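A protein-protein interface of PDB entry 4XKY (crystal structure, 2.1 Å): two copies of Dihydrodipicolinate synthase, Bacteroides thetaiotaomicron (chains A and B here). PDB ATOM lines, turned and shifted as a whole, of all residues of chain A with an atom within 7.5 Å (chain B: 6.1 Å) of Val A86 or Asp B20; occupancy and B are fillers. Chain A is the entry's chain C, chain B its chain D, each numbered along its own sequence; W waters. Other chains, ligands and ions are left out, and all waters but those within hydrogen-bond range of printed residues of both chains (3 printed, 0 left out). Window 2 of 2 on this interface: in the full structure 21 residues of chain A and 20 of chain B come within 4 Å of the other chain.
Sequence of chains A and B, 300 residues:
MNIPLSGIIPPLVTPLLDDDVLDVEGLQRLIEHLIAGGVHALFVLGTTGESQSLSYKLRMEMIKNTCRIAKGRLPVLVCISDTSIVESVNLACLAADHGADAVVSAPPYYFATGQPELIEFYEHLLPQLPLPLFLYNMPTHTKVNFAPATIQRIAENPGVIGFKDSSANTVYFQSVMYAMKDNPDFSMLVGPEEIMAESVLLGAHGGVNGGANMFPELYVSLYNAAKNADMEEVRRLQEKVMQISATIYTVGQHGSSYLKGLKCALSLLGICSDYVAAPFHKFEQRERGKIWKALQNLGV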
ATOM      1  N   TYR A  56      -9.167  16.750   4.675  1.00  0.00           N
ATOM      2  CA  TYR A  56      -9.710  17.109   5.965  1.00  0.00           C
ATOM      3  C   TYR A  56      -9.044  18.340   6.533  1.00  0.00           C
ATOM      4  O   TYR A  56      -9.719  19.270   6.965  1.00  0.00           O
ATOM      5  CB  TYR A  56      -9.571  15.980   6.967  1.00  0.00           C
ATOM      6  CG  TYR A  56     -10.678  16.067   7.962  1.00  0.00           C
ATOM      7  CD1 TYR A  56     -11.997  15.978   7.532  1.00  0.00           C
ATOM      8  CD2 TYR A  56     -10.432  16.297   9.317  1.00  0.00           C
ATOM      9  CE1 TYR A  56     -13.048  16.074   8.421  1.00  0.00           C
ATOM     10  CE2 TYR A  56     -11.482  16.398  10.218  1.00  0.00           C
ATOM     11  CZ  TYR A  56     -12.793  16.286   9.760  1.00  0.00           C
ATOM     12  OH  TYR A  56     -13.878  16.376  10.609  1.00  0.00           O
ATOM     13  N   ASP A  82     -20.652  15.222   4.848  1.00  0.00           N
ATOM     14  CA  ASP A  82     -19.513  14.350   4.691  1.00  0.00           C
ATOM     15  C   ASP A  82     -20.026  12.946   4.529  1.00  0.00           C
ATOM     16  O   ASP A  82     -21.103  12.611   5.035  1.00  0.00           O
ATOM     17  CB  ASP A  82     -18.585  14.416   5.905  1.00  0.00           C
ATOM     18  CG  ASP A  82     -17.219  13.815   5.613  1.00  0.00           C
ATOM     19  OD1 ASP A  82     -17.054  12.577   5.637  1.00  0.00           O
ATOM     20  OD2 ASP A  82     -16.310  14.602   5.319  1.00  0.00           O
ATOM     21  N   THR A  83     -19.271  12.120   3.811  1.00  0.00           N
ATOM     22  CA  THR A  83     -19.619  10.710   3.717  1.00  0.00           C
ATOM     23  C   THR A  83     -19.524  10.020   5.080  1.00  0.00           C
ATOM     24  O   THR A  83     -20.198   9.030   5.299  1.00  0.00           O
ATOM     25  CB  THR A  83     -18.734   9.944   2.695  1.00  0.00           C
ATOM     26  OG1 THR A  83     -17.354  10.066   3.053  1.00  0.00           O
ATOM     27  CG2 THR A  83     -18.953  10.481   1.286  1.00  0.00           C
ATOM     28  N   SER A  84     -18.666  10.524   5.969  1.00  0.00           N
ATOM     29  CA  SER A  84     -18.534   9.986   7.305  1.00  0.00           C
ATOM     30  C   SER A  84     -19.236  10.854   8.332  1.00  0.00           C
ATOM     31  O   SER A  84     -18.902  12.012   8.487  1.00  0.00           O
ATOM     32  CB  SER A  84     -17.074   9.910   7.721  1.00  0.00           C
ATOM     33  OG  SER A  84     -17.041   9.841   9.137  1.00  0.00           O
ATOM     34  N   ILE A  85     -20.146  10.274   9.095  1.00  0.00           N
ATOM     35  CA  ILE A  85     -20.914  11.059  10.079  1.00  0.00           C
ATOM     36  C   ILE A  85     -20.032  11.493  11.233  1.00  0.00           C
ATOM     37  O   ILE A  85     -20.143  12.616  11.718  1.00  0.00           O
ATOM     38  CB  ILE A  85     -22.158  10.286  10.583  1.00  0.00           C
ATOM     39  CG1 ILE A  85     -23.015   9.821   9.393  1.00  0.00           C
ATOM     40  CG2 ILE A  85     -23.006  11.147  11.520  1.00  0.00           C
ATOM     41  CD1 ILE A  85     -23.413  10.935   8.424  1.00  0.00           C
ATOM     42  N   VAL A  86     -19.122  10.625  11.659  1.00  0.00           N
ATOM     43  CA  VAL A  86     -18.111  11.010  12.659  1.00  0.00           C
ATOM     44  C   VAL A  86     -17.357  12.305  12.232  1.00  0.00           C
ATOM     45  O   VAL A  86     -17.246  13.277  13.010  1.00  0.00           O
ATOM     46  CB  VAL A  86     -17.142   9.830  12.900  1.00  0.00           C
ATOM     47  CG1 VAL A  86     -15.952  10.226  13.753  1.00  0.00           C
ATOM     48  CG2 VAL A  86     -17.905   8.670  13.531  1.00  0.00           C
ATOM     49  N   GLU A  87     -16.889  12.329  10.981  1.00  0.00           N
ATOM     50  CA  GLU A  87     -16.153  13.491  10.451  1.00  0.00           C
ATOM     51  C   GLU A  87     -17.081  14.696  10.371  1.00  0.00           C
ATOM     52  O   GLU A  87     -16.676  15.824  10.648  1.00  0.00           O
ATOM     53  CB  GLU A  87     -15.540  13.253   9.046  1.00  0.00           C
ATOM     54  CG  GLU A  87     -14.538  12.104   8.862  1.00  0.00           C
ATOM     55  CD  GLU A  87     -13.253  12.246   9.662  1.00  0.00           C
ATOM     56  OE1 GLU A  87     -13.036  13.314  10.274  1.00  0.00           O
ATOM     57  OE2 GLU A  87     -12.453  11.279   9.670  1.00  0.00           O
ATOM     58  N   SER A  88     -18.326  14.460   9.987  1.00  0.00           N
ATOM     59  CA  SER A  88     -19.323  15.529   9.992  1.00  0.00           C
ATOM     60  C   SER A  88     -19.485  16.183  11.384  1.00  0.00           C
ATOM     61  O   SER A  88     -19.473  17.414  11.522  1.00  0.00           O
ATOM     62  CB  SER A  88     -20.645  14.980   9.471  1.00  0.00           C
ATOM     63  OG  SER A  88     -21.598  15.997   9.414  1.00  0.00           O
ATOM     64  N   VAL A  89     -19.601  15.359  12.420  1.00  0.00           N
ATOM     65  CA  VAL A  89     -19.766  15.878  13.777  1.00  0.00           C
ATOM     66  C   VAL A  89     -18.505  16.666  14.179  1.00  0.00           C
ATOM     67  O   VAL A  89     -18.578  17.763  14.744  1.00  0.00           O
ATOM     68  CB  VAL A  89     -20.119  14.729  14.744  1.00  0.00           C
ATOM     69  CG1 VAL A  89     -20.076  15.193  16.199  1.00  0.00           C
ATOM     70  CG2 VAL A  89     -21.502  14.172  14.381  1.00  0.00           C
ATOM     71  N   ASN A  90     -17.348  16.131  13.840  1.00  0.00           N
ATOM     72  CA  ASN A  90     -16.114  16.823  14.133  1.00  0.00           C
ATOM     73  C   ASN A  90     -16.027  18.207  13.458  1.00  0.00           C
ATOM     74  O   ASN A  90     -15.639  19.170  14.101  1.00  0.00           O
ATOM     75  CB  ASN A  90     -14.943  15.928  13.790  1.00  0.00           C
ATOM     76  CG  ASN A  90     -13.627  16.553  14.141  1.00  0.00           C
ATOM     77  OD1 ASN A  90     -13.323  16.775  15.313  1.00  0.00           O
ATOM     78  ND2 ASN A  90     -12.839  16.863  13.126  1.00  0.00           N
ATOM     79  N   LEU A  91     -16.448  18.333  12.202  1.00  0.00           N
ATOM     80  CA  LEU A  91     -16.517  19.666  11.570  1.00  0.00           C
ATOM     81  C   LEU A  91     -17.486  20.586  12.307  1.00  0.00           C
ATOM     82  O   LEU A  91     -17.221  21.764  12.470  1.00  0.00           O
ATOM     83  CB  LEU A  91     -16.938  19.581  10.099  1.00  0.00           C
ATOM     84  CG  LEU A  91     -15.931  18.905   9.173  1.00  0.00           C
ATOM     85  CD1 LEU A  91     -16.580  18.672   7.812  1.00  0.00           C
ATOM     86  CD2 LEU A  91     -14.638  19.707   9.040  1.00  0.00           C
ATOM     87  N   ALA A  92     -18.614  20.046  12.746  1.00  0.00           N
ATOM     88  CA  ALA A  92     -19.581  20.817  13.528  1.00  0.00           C
ATOM     89  C   ALA A  92     -18.968  21.349  14.832  1.00  0.00           C
ATOM     90  O   ALA A  92     -19.206  22.495  15.196  1.00  0.00           O
ATOM     91  CB  ALA A  92     -20.815  19.979  13.830  1.00  0.00           C
ATOM     92  N   LEU A 125     -28.440  12.362  14.613  1.00  0.00           N
ATOM     93  CA  LEU A 125     -27.403  13.382  14.449  1.00  0.00           C
ATOM     94  C   LEU A 125     -27.568  14.583  15.383  1.00  0.00           C
ATOM     95  O   LEU A 125     -26.589  15.061  15.968  1.00  0.00           O
ATOM     96  CB  LEU A 125     -27.384  13.889  13.024  1.00  0.00           C
ATOM     97  CG  LEU A 125     -26.320  14.912  12.674  1.00  0.00           C
ATOM     98  CD1 LEU A 125     -24.928  14.304  12.809  1.00  0.00           C
ATOM     99  CD2 LEU A 125     -26.561  15.386  11.254  1.00  0.00           C
ATOM    100  N   GLN A 128     -25.886  15.269  18.748  1.00  0.00           N
ATOM    101  CA  GLN A 128     -24.448  15.365  18.699  1.00  0.00           C
ATOM    102  C   GLN A 128     -23.980  16.721  18.227  1.00  0.00           C
ATOM    103  O   GLN A 128     -22.795  16.994  18.296  1.00  0.00           O
ATOM    104  CB  GLN A 128     -23.861  14.309  17.772  1.00  0.00           C
ATOM    105  CG  GLN A 128     -24.313  12.896  18.067  1.00  0.00           C
ATOM    106  CD  GLN A 128     -23.677  11.918  17.110  1.00  0.00           C
ATOM    107  OE1 GLN A 128     -22.463  11.802  17.068  1.00  0.00           O
ATOM    108  NE2 GLN A 128     -24.490  11.200  16.353  1.00  0.00           N
ATOM    109  N   LEU B  16     -17.152  -3.456  13.492  1.00  0.00           N
ATOM    110  CA  LEU B  16     -17.233  -2.287  14.370  1.00  0.00           C
ATOM    111  C   LEU B  16     -17.918  -2.586  15.697  1.00  0.00           C
ATOM    112  O   LEU B  16     -18.973  -3.212  15.717  1.00  0.00           O
ATOM    113  CB  LEU B  16     -18.052  -1.202  13.677  1.00  0.00           C
ATOM    114  CG  LEU B  16     -17.568  -0.690  12.318  1.00  0.00           C
ATOM    115  CD1 LEU B  16     -18.614   0.280  11.778  1.00  0.00           C
ATOM    116  CD2 LEU B  16     -16.209  -0.026  12.439  1.00  0.00           C
ATOM    117  N   ASP B  18     -18.573   0.164  17.536  1.00  0.00           N
ATOM    118  CA  ASP B  18     -19.340   1.425  17.554  1.00  0.00           C
ATOM    119  C   ASP B  18     -18.974   2.251  16.295  1.00  0.00           C
ATOM    120  O   ASP B  18     -18.151   1.823  15.486  1.00  0.00           O
ATOM    121  CB  ASP B  18     -19.082   2.193  18.865  1.00  0.00           C
ATOM    122  CG  ASP B  18     -20.193   3.191  19.183  1.00  0.00           C
ATOM    123  OD1 ASP B  18     -21.153   3.296  18.407  1.00  0.00           O
ATOM    124  OD2 ASP B  18     -20.126   3.867  20.203  1.00  0.00           O
ATOM    125  N   ASP B  19     -19.616   3.397  16.088  1.00  0.00           N
ATOM    126  CA  ASP B  19     -19.450   4.122  14.820  1.00  0.00           C
ATOM    127  C   ASP B  19     -17.981   4.332  14.505  1.00  0.00           C
ATOM    128  O   ASP B  19     -17.543   4.204  13.355  1.00  0.00           O
ATOM    129  CB  ASP B  19     -20.123   5.491  14.877  1.00  0.00           C
ATOM    130  CG  ASP B  19     -21.607   5.386  14.870  1.00  0.00           C
ATOM    131  OD1 ASP B  19     -22.126   4.531  14.120  1.00  0.00           O
ATOM    132  OD2 ASP B  19     -22.237   6.125  15.637  1.00  0.00           O
ATOM    133  N   ASP B  20     -17.222   4.652  15.535  1.00  0.00           N
ATOM    134  CA  ASP B  20     -15.831   4.937  15.340  1.00  0.00           C
ATOM    135  C   ASP B  20     -14.889   3.991  16.089  1.00  0.00           C
ATOM    136  O   ASP B  20     -13.783   4.389  16.408  1.00  0.00           O
ATOM    137  CB  ASP B  20     -15.538   6.391  15.728  1.00  0.00           C
ATOM    138  CG  ASP B  20     -14.420   7.002  14.891  1.00  0.00           C
ATOM    139  OD1 ASP B  20     -14.234   6.571  13.731  1.00  0.00           O
ATOM    140  OD2 ASP B  20     -13.714   7.897  15.397  1.00  0.00           O
ATOM    141  N   VAL B  21     -15.304   2.761  16.373  1.00  0.00           N
ATOM    142  CA  VAL B  21     -14.438   1.829  17.112  1.00  0.00           C
ATOM    143  C   VAL B  21     -14.332   0.476  16.390  1.00  0.00           C
ATOM    144  O   VAL B  21     -15.338  -0.193  16.192  1.00  0.00           O
ATOM    145  CB  VAL B  21     -14.952   1.584  18.532  1.00  0.00           C
ATOM    146  CG1 VAL B  21     -14.013   0.622  19.258  1.00  0.00           C
ATOM    147  CG2 VAL B  21     -15.016   2.902  19.317  1.00  0.00           C
ATOM    148  N   LEU B  22     -13.112   0.085  16.031  1.00  0.00           N
ATOM    149  CA  LEU B  22     -12.850  -1.138  15.280  1.00  0.00           C
ATOM    150  C   LEU B  22     -12.994  -2.350  16.179  1.00  0.00           C
ATOM    151  O   LEU B  22     -12.474  -2.369  17.276  1.00  0.00           O
ATOM    152  CB  LEU B  22     -11.443  -1.099  14.681  1.00  0.00           C
ATOM    153  CG  LEU B  22     -11.005  -2.250  13.767  1.00  0.00           C
ATOM    154  CD1 LEU B  22     -11.797  -2.273  12.470  1.00  0.00           C
ATOM    155  CD2 LEU B  22      -9.535  -2.084  13.429  1.00  0.00           C
ATOM    156  N   SER B  53     -18.183   5.528   4.531  1.00  0.00           N
ATOM    157  CA  SER B  53     -18.936   5.914   5.701  1.00  0.00           C
ATOM    158  C   SER B  53     -18.101   5.875   6.999  1.00  0.00           C
ATOM    159  O   SER B  53     -18.567   6.338   8.037  1.00  0.00           O
ATOM    160  CB  SER B  53     -20.231   5.083   5.769  1.00  0.00           C
ATOM    161  OG  SER B  53     -19.972   3.776   6.194  1.00  0.00           O
ATOM    162  N   LEU B  54     -16.863   5.371   6.938  1.00  0.00           N
ATOM    163  CA  LEU B  54     -15.988   5.352   8.116  1.00  0.00           C
ATOM    164  C   LEU B  54     -15.133   6.619   8.199  1.00  0.00           C
ATOM    165  O   LEU B  54     -14.806   7.200   7.179  1.00  0.00           O
ATOM    166  CB  LEU B  54     -15.075   4.113   8.031  1.00  0.00           C
ATOM    167  CG  LEU B  54     -15.858   2.797   8.030  1.00  0.00           C
ATOM    168  CD1 LEU B  54     -14.924   1.629   8.151  1.00  0.00           C
ATOM    169  CD2 LEU B  54     -16.896   2.732   9.138  1.00  0.00           C
ATOM    170  N   SER B  55     -14.740   7.022   9.398  1.00  0.00           N
ATOM    171  CA  SER B  55     -13.761   8.102   9.564  1.00  0.00           C
ATOM    172  C   SER B  55     -12.378   7.763   8.986  1.00  0.00           C
ATOM    173  O   SER B  55     -12.064   6.582   8.789  1.00  0.00           O
ATOM    174  CB  SER B  55     -13.598   8.401  11.034  1.00  0.00           C
ATOM    175  OG  SER B  55     -12.893   7.375  11.707  1.00  0.00           O
ATOM    176  N   TYR B  56     -11.589   8.805   8.743  1.00  0.00           N
ATOM    177  CA  TYR B  56     -10.222   8.648   8.283  1.00  0.00           C
ATOM    178  C   TYR B  56      -9.440   7.764   9.226  1.00  0.00           C
ATOM    179  O   TYR B  56      -8.776   6.830   8.794  1.00  0.00           O
ATOM    180  CB  TYR B  56      -9.502   9.994   8.155  1.00  0.00           C
ATOM    181  CG  TYR B  56      -8.411   9.896   7.129  1.00  0.00           C
ATOM    182  CD1 TYR B  56      -8.725   9.535   5.840  1.00  0.00           C
ATOM    183  CD2 TYR B  56      -7.070  10.102   7.451  1.00  0.00           C
ATOM    184  CE1 TYR B  56      -7.754   9.397   4.882  1.00  0.00           C
ATOM    185  CE2 TYR B  56      -6.085   9.974   6.483  1.00  0.00           C
ATOM    186  CZ  TYR B  56      -6.451   9.619   5.203  1.00  0.00           C
ATOM    187  OH  TYR B  56      -5.532   9.487   4.207  1.00  0.00           O
ATOM    188  N   LYS B  57      -9.545   8.060  10.517  1.00  0.00           N
ATOM    189  CA  LYS B  57      -8.855   7.311  11.556  1.00  0.00           C
ATOM    190  C   LYS B  57      -9.200   5.819  11.490  1.00  0.00           C
ATOM    191  O   LYS B  57      -8.329   4.968  11.625  1.00  0.00           O
ATOM    192  CB  LYS B  57      -9.153   7.867  12.964  1.00  0.00           C
ATOM    193  CG  LYS B  57      -8.778   6.898  14.088  1.00  0.00           C
ATOM    194  CD  LYS B  57      -8.730   7.501  15.494  1.00  0.00           C
ATOM    195  CE  LYS B  57     -10.090   7.566  16.196  1.00  0.00           C
ATOM    196  NZ  LYS B  57     -10.865   6.288  16.238  1.00  0.00           N
ATOM    197  N   LEU B  58     -10.470   5.513  11.281  1.00  0.00           N
ATOM    198  CA  LEU B  58     -10.904   4.146  11.317  1.00  0.00           C
ATOM    199  C   LEU B  58     -10.470   3.394  10.064  1.00  0.00           C
ATOM    200  O   LEU B  58     -10.121   2.213  10.128  1.00  0.00           O
ATOM    201  CB  LEU B  58     -12.410   4.117  11.466  1.00  0.00           C
ATOM    202  CG  LEU B  58     -13.033   2.797  11.850  1.00  0.00           C
ATOM    203  CD1 LEU B  58     -12.356   2.148  13.040  1.00  0.00           C
ATOM    204  CD2 LEU B  58     -14.483   3.059  12.193  1.00  0.00           C
ATOM    205  N   GLU B  61      -6.995   2.444  10.743  1.00  0.00           N
ATOM    206  CA  GLU B  61      -6.888   1.328  11.688  1.00  0.00           C
ATOM    207  C   GLU B  61      -7.232  -0.007  11.018  1.00  0.00           C
ATOM    208  O   GLU B  61      -6.619  -1.042  11.319  1.00  0.00           O
ATOM    209  CB  GLU B  61      -7.776   1.528  12.938  1.00  0.00           C
ATOM    210  CG  GLU B  61      -7.336   2.705  13.797  1.00  0.00           C
ATOM    211  CD  GLU B  61      -8.252   2.982  14.983  1.00  0.00           C
ATOM    212  OE1 GLU B  61      -9.270   2.276  15.149  1.00  0.00           O
ATOM    213  OE2 GLU B  61      -7.944   3.908  15.765  1.00  0.00           O
HETATM  214  O   HOH W   1     -20.866   7.629   8.402  1.00  0.00           O
HETATM  215  O   HOH W   2     -10.889  10.321  11.817  1.00  0.00           O
HETATM  216  O   HOH W   3     -17.997   7.634  10.531  1.00  0.00           O
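Of the 14 printed residues of chain A, 4 touch a printed residue of chain B.
Along chain A the printed residues that touch a printed residue of chain B span positions 83 to 87.
The side-chain amino group (NZ) of Lys B57 is in salt-bridge range of the side-chain carboxylate (OD2) of Asp B20.
The side-chain hydroxyl of Ser B55 lies within hydrogen-bond range of the side-chain carboxylate of Asp B20.
The side-chain hydroxyl (OG) of Ser A84 sits close to the backbone NH (N) of Val A86, at 3.4 Å.
N of Ser A84 sits at hydrogen-bond distance from OD1 of Asp A82, at 2.6 Å.
The side-chain hydroxyl (OG) of Ser B55 sits at hydrogen-bond distance from the backbone NH (N) of Leu B58 (3.1 Å).
The side-chain hydroxyl (OG) of Ser A84 is in hydrogen-bond range of the backbone NH (N) of Glu A87 (3.1 Å).
The backbone NH (N) of Tyr B56 lies within hydrogen-bond range of the side-chain carboxylate (OE2) of Glu A87, at 2.8 Å.
Printed residues of chain B within 4 Å of Val A86: Asp B20 (3.6 Å).
Asp B20 touches just one residue of chain A: Val A86.
Printed residues of chain B within 4 Å of Thr A83: Ser B53.
Of the printed residues of chain A, Ser B53 touches Thr A83 (3.4 Å) and Ser A84 (3.7 Å).
Of the printed residues of chain A, Tyr B56 touches Glu A87.
Of the printed residues of chain B, Glu A87 touches Ser B55 (3.4 Å) and Tyr B56 (2.8 Å).
Printed residues of chain A within 4 Å of Ser B55: Ser A84 and Glu A87.
Leu A125 touches none of the printed residues of chain B.
The nearest printed residue of chain A that does not touch Leu B54 is Glu A87 (5.2 Å).
CA of Ser B53 touches O of Thr A83 (3.4 Å).
Ser B53 touches Ser A84.
O of Leu B54 touches CB of Ser A84, 3.6 Å away.
Ser A84 touches Ser B55.
Val A86 touches Asp B20.
Glu A87 touches Ser B55.
Water W1 lies within hydrogen-bond range of the backbone carbonyl oxygen of Ser B53 (2.7 Å), the backbone NH of Ile A85 (2.8 Å) and the backbone carbonyl oxygen of Thr A83 (3.5 Å).
Water W3 lies within hydrogen-bond range of the side-chain hydroxyl of Ser A84, the backbone carbonyl oxygen of Ser B53 and the backbone NH of Val A86.
Water W2 lies within hydrogen-bond range of OE2 of Glu A87 (2.8 Å), N of Lys B57 (2.9 Å) and N of Tyr B56 (3.5 Å).
Position printed for both chains: 56.
Of the 7 pairs that touch across the chains among the printed residues, none has its exchanged pair printed and touching as well.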
